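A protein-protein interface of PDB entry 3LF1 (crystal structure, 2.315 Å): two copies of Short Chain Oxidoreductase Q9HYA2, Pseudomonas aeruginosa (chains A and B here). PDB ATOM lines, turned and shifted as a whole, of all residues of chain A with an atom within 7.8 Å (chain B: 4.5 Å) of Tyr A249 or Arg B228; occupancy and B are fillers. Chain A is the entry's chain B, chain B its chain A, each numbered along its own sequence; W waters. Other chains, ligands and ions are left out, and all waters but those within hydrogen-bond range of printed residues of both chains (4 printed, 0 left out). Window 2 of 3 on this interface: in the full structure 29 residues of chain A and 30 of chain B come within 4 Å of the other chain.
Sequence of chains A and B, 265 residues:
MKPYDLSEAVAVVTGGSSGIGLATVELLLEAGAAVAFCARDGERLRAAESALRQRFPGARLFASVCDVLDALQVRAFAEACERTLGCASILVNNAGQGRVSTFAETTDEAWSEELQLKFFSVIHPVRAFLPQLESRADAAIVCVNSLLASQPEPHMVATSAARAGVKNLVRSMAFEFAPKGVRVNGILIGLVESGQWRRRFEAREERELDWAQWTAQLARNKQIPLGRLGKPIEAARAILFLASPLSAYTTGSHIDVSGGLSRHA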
ATOM      1  N   ARG A 183     -24.133 -11.151 -33.500  1.00  0.00           N
ATOM      2  CA  ARG A 183     -23.843 -11.583 -32.144  1.00  0.00           C
ATOM      3  C   ARG A 183     -23.316 -13.022 -32.176  1.00  0.00           C
ATOM      4  O   ARG A 183     -23.697 -13.821 -33.030  1.00  0.00           O
ATOM      5  CB  ARG A 183     -25.089 -11.449 -31.241  1.00  0.00           C
ATOM      6  CG  ARG A 183     -25.586 -10.004 -31.091  1.00  0.00           C
ATOM      7  CD  ARG A 183     -26.661  -9.877 -30.003  1.00  0.00           C
ATOM      8  NE  ARG A 183     -27.852 -10.638 -30.341  1.00  0.00           N
ATOM      9  CZ  ARG A 183     -28.181 -11.799 -29.784  1.00  0.00           C
ATOM     10  NH1 ARG A 183     -27.414 -12.342 -28.848  1.00  0.00           N
ATOM     11  NH2 ARG A 183     -29.266 -12.428 -30.182  1.00  0.00           N
ATOM     12  N   ASN A 185     -22.609 -16.174 -29.395  1.00  0.00           N
ATOM     13  CA  ASN A 185     -22.579 -16.755 -28.056  1.00  0.00           C
ATOM     14  C   ASN A 185     -22.489 -18.273 -28.111  1.00  0.00           C
ATOM     15  O   ASN A 185     -22.406 -18.865 -29.182  1.00  0.00           O
ATOM     16  CB  ASN A 185     -23.820 -16.357 -27.248  1.00  0.00           C
ATOM     17  CG  ASN A 185     -23.956 -14.846 -27.078  1.00  0.00           C
ATOM     18  OD1 ASN A 185     -23.290 -14.229 -26.232  1.00  0.00           O
ATOM     19  ND2 ASN A 185     -24.822 -14.248 -27.883  1.00  0.00           N
ATOM     20  N   SER A 244     -32.216 -15.636 -30.614  1.00  0.00           N
ATOM     21  CA  SER A 244     -33.279 -14.672 -30.911  1.00  0.00           C
ATOM     22  C   SER A 244     -32.970 -13.248 -30.426  1.00  0.00           C
ATOM     23  O   SER A 244     -31.980 -13.029 -29.727  1.00  0.00           O
ATOM     24  CB  SER A 244     -34.573 -15.148 -30.279  1.00  0.00           C
ATOM     25  OG  SER A 244     -34.549 -14.884 -28.888  1.00  0.00           O
ATOM     26  N   PRO A 245     -33.810 -12.270 -30.815  1.00  0.00           N
ATOM     27  CA  PRO A 245     -33.716 -10.884 -30.318  1.00  0.00           C
ATOM     28  C   PRO A 245     -33.922 -10.738 -28.813  1.00  0.00           C
ATOM     29  O   PRO A 245     -33.646  -9.676 -28.265  1.00  0.00           O
ATOM     30  CB  PRO A 245     -34.844 -10.168 -31.068  1.00  0.00           C
ATOM     31  CG  PRO A 245     -34.919 -10.903 -32.383  1.00  0.00           C
ATOM     32  CD  PRO A 245     -34.700 -12.366 -31.993  1.00  0.00           C
ATOM     33  N   LEU A 246     -34.403 -11.784 -28.151  1.00  0.00           N
ATOM     34  CA  LEU A 246     -34.566 -11.730 -26.705  1.00  0.00           C
ATOM     35  C   LEU A 246     -33.219 -11.442 -26.031  1.00  0.00           C
ATOM     36  O   LEU A 246     -33.172 -10.857 -24.944  1.00  0.00           O
ATOM     37  CB  LEU A 246     -35.171 -13.036 -26.171  1.00  0.00           C
ATOM     38  CG  LEU A 246     -36.540 -13.500 -26.708  1.00  0.00           C
ATOM     39  CD1 LEU A 246     -36.940 -14.886 -26.206  1.00  0.00           C
ATOM     40  CD2 LEU A 246     -37.636 -12.499 -26.358  1.00  0.00           C
ATOM     41  N   SER A 247     -32.119 -11.838 -26.664  1.00  0.00           N
ATOM     42  CA  SER A 247     -30.804 -11.605 -26.052  1.00  0.00           C
ATOM     43  C   SER A 247     -29.974 -10.584 -26.834  1.00  0.00           C
ATOM     44  O   SER A 247     -28.751 -10.723 -26.982  1.00  0.00           O
ATOM     45  CB  SER A 247     -30.047 -12.924 -25.915  1.00  0.00           C
ATOM     46  OG  SER A 247     -29.894 -13.538 -27.184  1.00  0.00           O
ATOM     47  N   ALA A 248     -30.656  -9.552 -27.321  1.00  0.00           N
ATOM     48  CA  ALA A 248     -30.045  -8.557 -28.191  1.00  0.00           C
ATOM     49  C   ALA A 248     -28.829  -7.831 -27.586  1.00  0.00           C
ATOM     50  O   ALA A 248     -28.026  -7.257 -28.307  1.00  0.00           O
ATOM     51  CB  ALA A 248     -31.116  -7.551 -28.650  1.00  0.00           C
ATOM     52  N   TYR A 249     -28.677  -7.845 -26.267  1.00  0.00           N
ATOM     53  CA  TYR A 249     -27.535  -7.141 -25.669  1.00  0.00           C
ATOM     54  C   TYR A 249     -26.488  -8.110 -25.093  1.00  0.00           C
ATOM     55  O   TYR A 249     -25.668  -7.735 -24.236  1.00  0.00           O
ATOM     56  CB  TYR A 249     -28.009  -6.152 -24.606  1.00  0.00           C
ATOM     57  CG  TYR A 249     -27.045  -5.023 -24.355  1.00  0.00           C
ATOM     58  CD1 TYR A 249     -26.652  -4.171 -25.394  1.00  0.00           C
ATOM     59  CD2 TYR A 249     -26.533  -4.787 -23.073  1.00  0.00           C
ATOM     60  CE1 TYR A 249     -25.765  -3.120 -25.157  1.00  0.00           C
ATOM     61  CE2 TYR A 249     -25.657  -3.742 -22.833  1.00  0.00           C
ATOM     62  CZ  TYR A 249     -25.277  -2.915 -23.874  1.00  0.00           C
ATOM     63  OH  TYR A 249     -24.408  -1.879 -23.623  1.00  0.00           O
ATOM     64  N   THR A 250     -26.525  -9.352 -25.577  1.00  0.00           N
ATOM     65  CA  THR A 250     -25.650 -10.410 -25.085  1.00  0.00           C
ATOM     66  C   THR A 250     -24.784 -10.963 -26.214  1.00  0.00           C
ATOM     67  O   THR A 250     -25.288 -11.577 -27.143  1.00  0.00           O
ATOM     68  CB  THR A 250     -26.482 -11.567 -24.508  1.00  0.00           C
ATOM     69  OG1 THR A 250     -27.257 -11.101 -23.389  1.00  0.00           O
ATOM     70  CG2 THR A 250     -25.588 -12.724 -24.078  1.00  0.00           C
ATOM     71  N   THR A 251     -23.477 -10.766 -26.134  1.00  0.00           N
ATOM     72  CA  THR A 251     -22.598 -11.335 -27.136  1.00  0.00           C
ATOM     73  C   THR A 251     -21.236 -11.650 -26.527  1.00  0.00           C
ATOM     74  O   THR A 251     -20.774 -10.964 -25.607  1.00  0.00           O
ATOM     75  CB  THR A 251     -22.464 -10.425 -28.380  1.00  0.00           C
ATOM     76  OG1 THR A 251     -21.752 -11.118 -29.420  1.00  0.00           O
ATOM     77  CG2 THR A 251     -21.751  -9.124 -28.027  1.00  0.00           C
ATOM     78  N   GLY A 252     -20.618 -12.721 -27.010  1.00  0.00           N
ATOM     79  CA  GLY A 252     -19.318 -13.139 -26.504  1.00  0.00           C
ATOM     80  C   GLY A 252     -19.410 -13.818 -25.151  1.00  0.00           C
ATOM     81  O   GLY A 252     -18.444 -13.803 -24.386  1.00  0.00           O
ATOM     82  N   SER A 253     -20.574 -14.402 -24.849  1.00  0.00           N
ATOM     83  CA  SER A 253     -20.813 -15.046 -23.556  1.00  0.00           C
ATOM     84  C   SER A 253     -21.300 -16.485 -23.712  1.00  0.00           C
ATOM     85  O   SER A 253     -21.453 -16.988 -24.828  1.00  0.00           O
ATOM     86  CB  SER A 253     -21.850 -14.254 -22.753  1.00  0.00           C
ATOM     87  OG  SER A 253     -23.170 -14.580 -23.185  1.00  0.00           O
ATOM     88  N   LEU B 191     -23.554  -1.441 -19.049  1.00  0.00           N
ATOM     89  CA  LEU B 191     -24.119  -0.104 -18.891  1.00  0.00           C
ATOM     90  C   LEU B 191     -25.528  -0.074 -19.480  1.00  0.00           C
ATOM     91  O   LEU B 191     -25.708  -0.317 -20.672  1.00  0.00           O
ATOM     92  CB  LEU B 191     -23.227   0.951 -19.565  1.00  0.00           C
ATOM     93  CG  LEU B 191     -21.801   1.093 -19.011  1.00  0.00           C
ATOM     94  CD1 LEU B 191     -21.054   2.278 -19.613  1.00  0.00           C
ATOM     95  CD2 LEU B 191     -21.847   1.246 -17.524  1.00  0.00           C
ATOM     96  N   ALA B 219     -21.018   4.934 -25.412  1.00  0.00           N
ATOM     97  CA  ALA B 219     -20.766   3.508 -25.526  1.00  0.00           C
ATOM     98  C   ALA B 219     -19.446   3.258 -26.250  1.00  0.00           C
ATOM     99  O   ALA B 219     -18.730   2.300 -25.963  1.00  0.00           O
ATOM    100  CB  ALA B 219     -21.918   2.814 -26.245  1.00  0.00           C
ATOM    101  N   ILE B 224     -17.817  -0.505 -25.725  1.00  0.00           N
ATOM    102  CA  ILE B 224     -18.833  -1.541 -25.779  1.00  0.00           C
ATOM    103  C   ILE B 224     -19.004  -2.001 -27.222  1.00  0.00           C
ATOM    104  O   ILE B 224     -19.464  -1.243 -28.068  1.00  0.00           O
ATOM    105  CB  ILE B 224     -20.174  -1.046 -25.228  1.00  0.00           C
ATOM    106  CG1 ILE B 224     -19.983  -0.473 -23.823  1.00  0.00           C
ATOM    107  CG2 ILE B 224     -21.177  -2.177 -25.214  1.00  0.00           C
ATOM    108  CD1 ILE B 224     -21.263  -0.006 -23.167  1.00  0.00           C
ATOM    109  N   LEU B 226     -21.149  -3.727 -28.911  1.00  0.00           N
ATOM    110  CA  LEU B 226     -22.453  -3.485 -29.532  1.00  0.00           C
ATOM    111  C   LEU B 226     -22.734  -2.003 -29.806  1.00  0.00           C
ATOM    112  O   LEU B 226     -23.705  -1.681 -30.461  1.00  0.00           O
ATOM    113  CB  LEU B 226     -23.589  -4.095 -28.708  1.00  0.00           C
ATOM    114  CG  LEU B 226     -23.662  -5.625 -28.726  1.00  0.00           C
ATOM    115  CD1 LEU B 226     -24.955  -6.102 -28.089  1.00  0.00           C
ATOM    116  CD2 LEU B 226     -23.557  -6.167 -30.146  1.00  0.00           C
ATOM    117  N   GLY B 227     -21.887  -1.114 -29.287  1.00  0.00           N
ATOM    118  CA  GLY B 227     -21.943   0.294 -29.635  1.00  0.00           C
ATOM    119  C   GLY B 227     -23.189   1.043 -29.184  1.00  0.00           C
ATOM    120  O   GLY B 227     -23.643   1.945 -29.874  1.00  0.00           O
ATOM    121  N   ARG B 228     -23.724   0.683 -28.018  1.00  0.00           N
ATOM    122  CA  ARG B 228     -24.888   1.356 -27.433  1.00  0.00           C
ATOM    123  C   ARG B 228     -25.086   0.895 -25.997  1.00  0.00           C
ATOM    124  O   ARG B 228     -24.550  -0.134 -25.587  1.00  0.00           O
ATOM    125  CB  ARG B 228     -26.161   1.046 -28.229  1.00  0.00           C
ATOM    126  CG  ARG B 228     -26.583  -0.425 -28.186  1.00  0.00           C
ATOM    127  CD  ARG B 228     -27.988  -0.603 -28.728  1.00  0.00           C
ATOM    128  NE  ARG B 228     -28.359  -2.009 -28.888  1.00  0.00           N
ATOM    129  CZ  ARG B 228     -28.994  -2.725 -27.966  1.00  0.00           C
ATOM    130  NH1 ARG B 228     -29.323  -2.172 -26.796  1.00  0.00           N
ATOM    131  NH2 ARG B 228     -29.294  -3.997 -28.214  1.00  0.00           N
ATOM    132  N   LEU B 229     -25.856   1.662 -25.238  1.00  0.00           N
ATOM    133  CA  LEU B 229     -26.269   1.259 -23.906  1.00  0.00           C
ATOM    134  C   LEU B 229     -27.325   0.148 -23.988  1.00  0.00           C
ATOM    135  O   LEU B 229     -28.022   0.014 -24.990  1.00  0.00           O
ATOM    136  CB  LEU B 229     -26.824   2.463 -23.153  1.00  0.00           C
ATOM    137  CG  LEU B 229     -25.887   3.070 -22.103  1.00  0.00           C
ATOM    138  CD1 LEU B 229     -24.471   3.243 -22.663  1.00  0.00           C
ATOM    139  CD2 LEU B 229     -26.460   4.392 -21.619  1.00  0.00           C
ATOM    140  N   GLY B 230     -27.424  -0.666 -22.946  1.00  0.00           N
ATOM    141  CA  GLY B 230     -28.460  -1.676 -22.887  1.00  0.00           C
ATOM    142  C   GLY B 230     -29.791  -1.023 -22.538  1.00  0.00           C
ATOM    143  O   GLY B 230     -29.829   0.102 -22.037  1.00  0.00           O
ATOM    144  N   LYS B 231     -30.886  -1.716 -22.836  1.00  0.00           N
ATOM    145  CA  LYS B 231     -32.202  -1.249 -22.434  1.00  0.00           C
ATOM    146  C   LYS B 231     -32.716  -2.118 -21.297  1.00  0.00           C
ATOM    147  O   LYS B 231     -32.527  -3.333 -21.312  1.00  0.00           O
ATOM    148  CB  LYS B 231     -33.159  -1.233 -23.626  1.00  0.00           C
ATOM    149  CG  LYS B 231     -32.788  -0.205 -24.685  1.00  0.00           C
ATOM    150  CD  LYS B 231     -33.917   0.007 -25.671  1.00  0.00           C
ATOM    151  CE  LYS B 231     -33.608   1.155 -26.629  1.00  0.00           C
ATOM    152  NZ  LYS B 231     -33.137   2.380 -25.927  1.00  0.00           N
ATOM    153  N   GLU B 234     -34.089  -5.410 -21.920  1.00  0.00           N
ATOM    154  CA  GLU B 234     -33.113  -6.447 -22.277  1.00  0.00           C
ATOM    155  C   GLU B 234     -32.559  -7.172 -21.050  1.00  0.00           C
ATOM    156  O   GLU B 234     -32.451  -8.397 -21.044  1.00  0.00           O
ATOM    157  CB  GLU B 234     -31.992  -5.851 -23.141  1.00  0.00           C
ATOM    158  CG  GLU B 234     -32.503  -5.217 -24.439  1.00  0.00           C
ATOM    159  CD  GLU B 234     -31.430  -4.522 -25.209  1.00  0.00           C
ATOM    160  OE1 GLU B 234     -30.621  -3.808 -24.586  1.00  0.00           O
ATOM    161  OE2 GLU B 234     -31.395  -4.688 -26.439  1.00  0.00           O
ATOM    162  N   VAL B 257     -25.167  -9.655 -19.750  1.00  0.00           N
ATOM    163  CA  VAL B 257     -25.965  -8.667 -20.463  1.00  0.00           C
ATOM    164  C   VAL B 257     -25.216  -7.325 -20.539  1.00  0.00           C
ATOM    165  O   VAL B 257     -25.710  -6.296 -20.081  1.00  0.00           O
ATOM    166  CB  VAL B 257     -27.364  -8.493 -19.816  1.00  0.00           C
ATOM    167  CG1 VAL B 257     -28.293  -7.715 -20.756  1.00  0.00           C
ATOM    168  CG2 VAL B 257     -27.975  -9.843 -19.497  1.00  0.00           C
ATOM    169  N   SER B 258     -24.025  -7.341 -21.127  1.00  0.00           N
ATOM    170  CA  SER B 258     -23.146  -6.169 -21.075  1.00  0.00           C
ATOM    171  C   SER B 258     -22.798  -5.662 -22.462  1.00  0.00           C
ATOM    172  O   SER B 258     -22.021  -4.728 -22.607  1.00  0.00           O
ATOM    173  CB  SER B 258     -21.857  -6.487 -20.295  1.00  0.00           C
ATOM    174  OG  SER B 258     -21.014  -7.408 -20.987  1.00  0.00           O
ATOM    175  N   GLY B 259     -23.378  -6.274 -23.491  1.00  0.00           N
ATOM    176  CA  GLY B 259     -23.100  -5.858 -24.852  1.00  0.00           C
ATOM    177  C   GLY B 259     -21.683  -6.177 -25.308  1.00  0.00           C
ATOM    178  O   GLY B 259     -21.165  -5.516 -26.210  1.00  0.00           O
HETATM  179  O   HOH W   1     -19.269  -9.666 -22.796  1.00  0.00           O
HETATM  180  O   HOH W   2     -22.355  -9.484 -23.603  1.00  0.00           O
HETATM  181  O   HOH W   3     -31.744 -10.345 -22.841  1.00  0.00           O
HETATM  182  O   HOH W   4     -22.634  -2.377 -21.468  1.00  0.00           O
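Printed residues of chain A that touch a printed residue of chain B: Ala A248 and Tyr A249. Among the printed residues, 13 pairs touch across the chains.
CD1 of Leu B226 touches O of Ala A248 (3.3 Å). Ala A248 touches Glu B234. OH of Tyr A249 touches O of Leu B191, 3.6 Å away. CG2 of Ile B224 touches OH of Tyr A249 (3.6 Å). Tyr A249 touches Leu B226 (CA to CD1, 3.7 Å). Tyr A249 touches Leu B229 (OH to C, 3.6 Å). Glu B234 touches Tyr A249. Tyr A249 touches Val B257. CE2 of Tyr A249 touches C of Ser B258 (3.5 Å).
No position is printed for both chains. Of the 13 pairs that touch across the chains among the printed residues, none has its exchanged pair printed and touching as well.
The side-chain carboxylate of Glu B234 lies within salt-bridge range of the guanidinium group of Arg B228 (2.8 Å). N of Gly B230 is in hydrogen-bond range of O of Leu B191, 2.9 Å away. The side-chain carboxylate (OE1) of Glu B234 is in hydrogen-bond range of the backbone NH (N) of Lys B231 (2.7 Å). The backbone carbonyl oxygen (O) of Ala B219 lies within hydrogen-bond range of the backbone NH (N) of Ile B224, 3.0 Å away. O of Gly B259 sits at hydrogen-bond distance from N of Leu B226, at 3.2 Å.
Water W3 bridges the backbone carbonyl oxygen of Leu A246 (2.6 Å) and the backbone carbonyl oxygen of Glu B234 (2.7 Å). Water W4 lies within hydrogen-bond range of the backbone carbonyl oxygen (O) of Ser B258 (2.7 Å), the backbone NH (N) of Leu B191 (2.8 Å) and the side-chain hydroxyl (OH) of Tyr A249 (2.8 Å). Water W2 lies within hydrogen-bond range of O of Thr A251 and N of Gly B259. Water W1 bridges OG of Ser B258 and O of Thr A251.
N of Gly B259 is in hydrogen-bond range of O of Tyr A249. N of Gly B230 lies close to OH of Tyr A249, 3.3 Å away. NH2 of Arg B228 is in hydrogen-bond range of O of Ala A248. O of Arg B228 sits at hydrogen-bond distance from OH of Tyr A249.
Tyr A249 touches just these residues of chain B: Leu B191, Ile B224, Leu B226, Arg B228, Leu B229, Gly B230, Glu B234, Val B257, Ser B258 and Gly B259. Printed residues of chain A within 4 Å of Gly B259: Tyr A249 (2.8 Å). Printed residues of chain A within 4 Å of Val B257: Tyr A249. Of the printed residues of chain A, Leu B191 touches Tyr A249 (3.6 Å). Of the printed residues of chain A, Leu B226 touches Ala A248 and Tyr A249. Gly A252 touches none of the printed residues of chain B. Ser A253 touches none of the printed residues of chain B. The nearest printed residue of chain A that does not touch Glu B234 is Leu A246 (4.7 Å).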
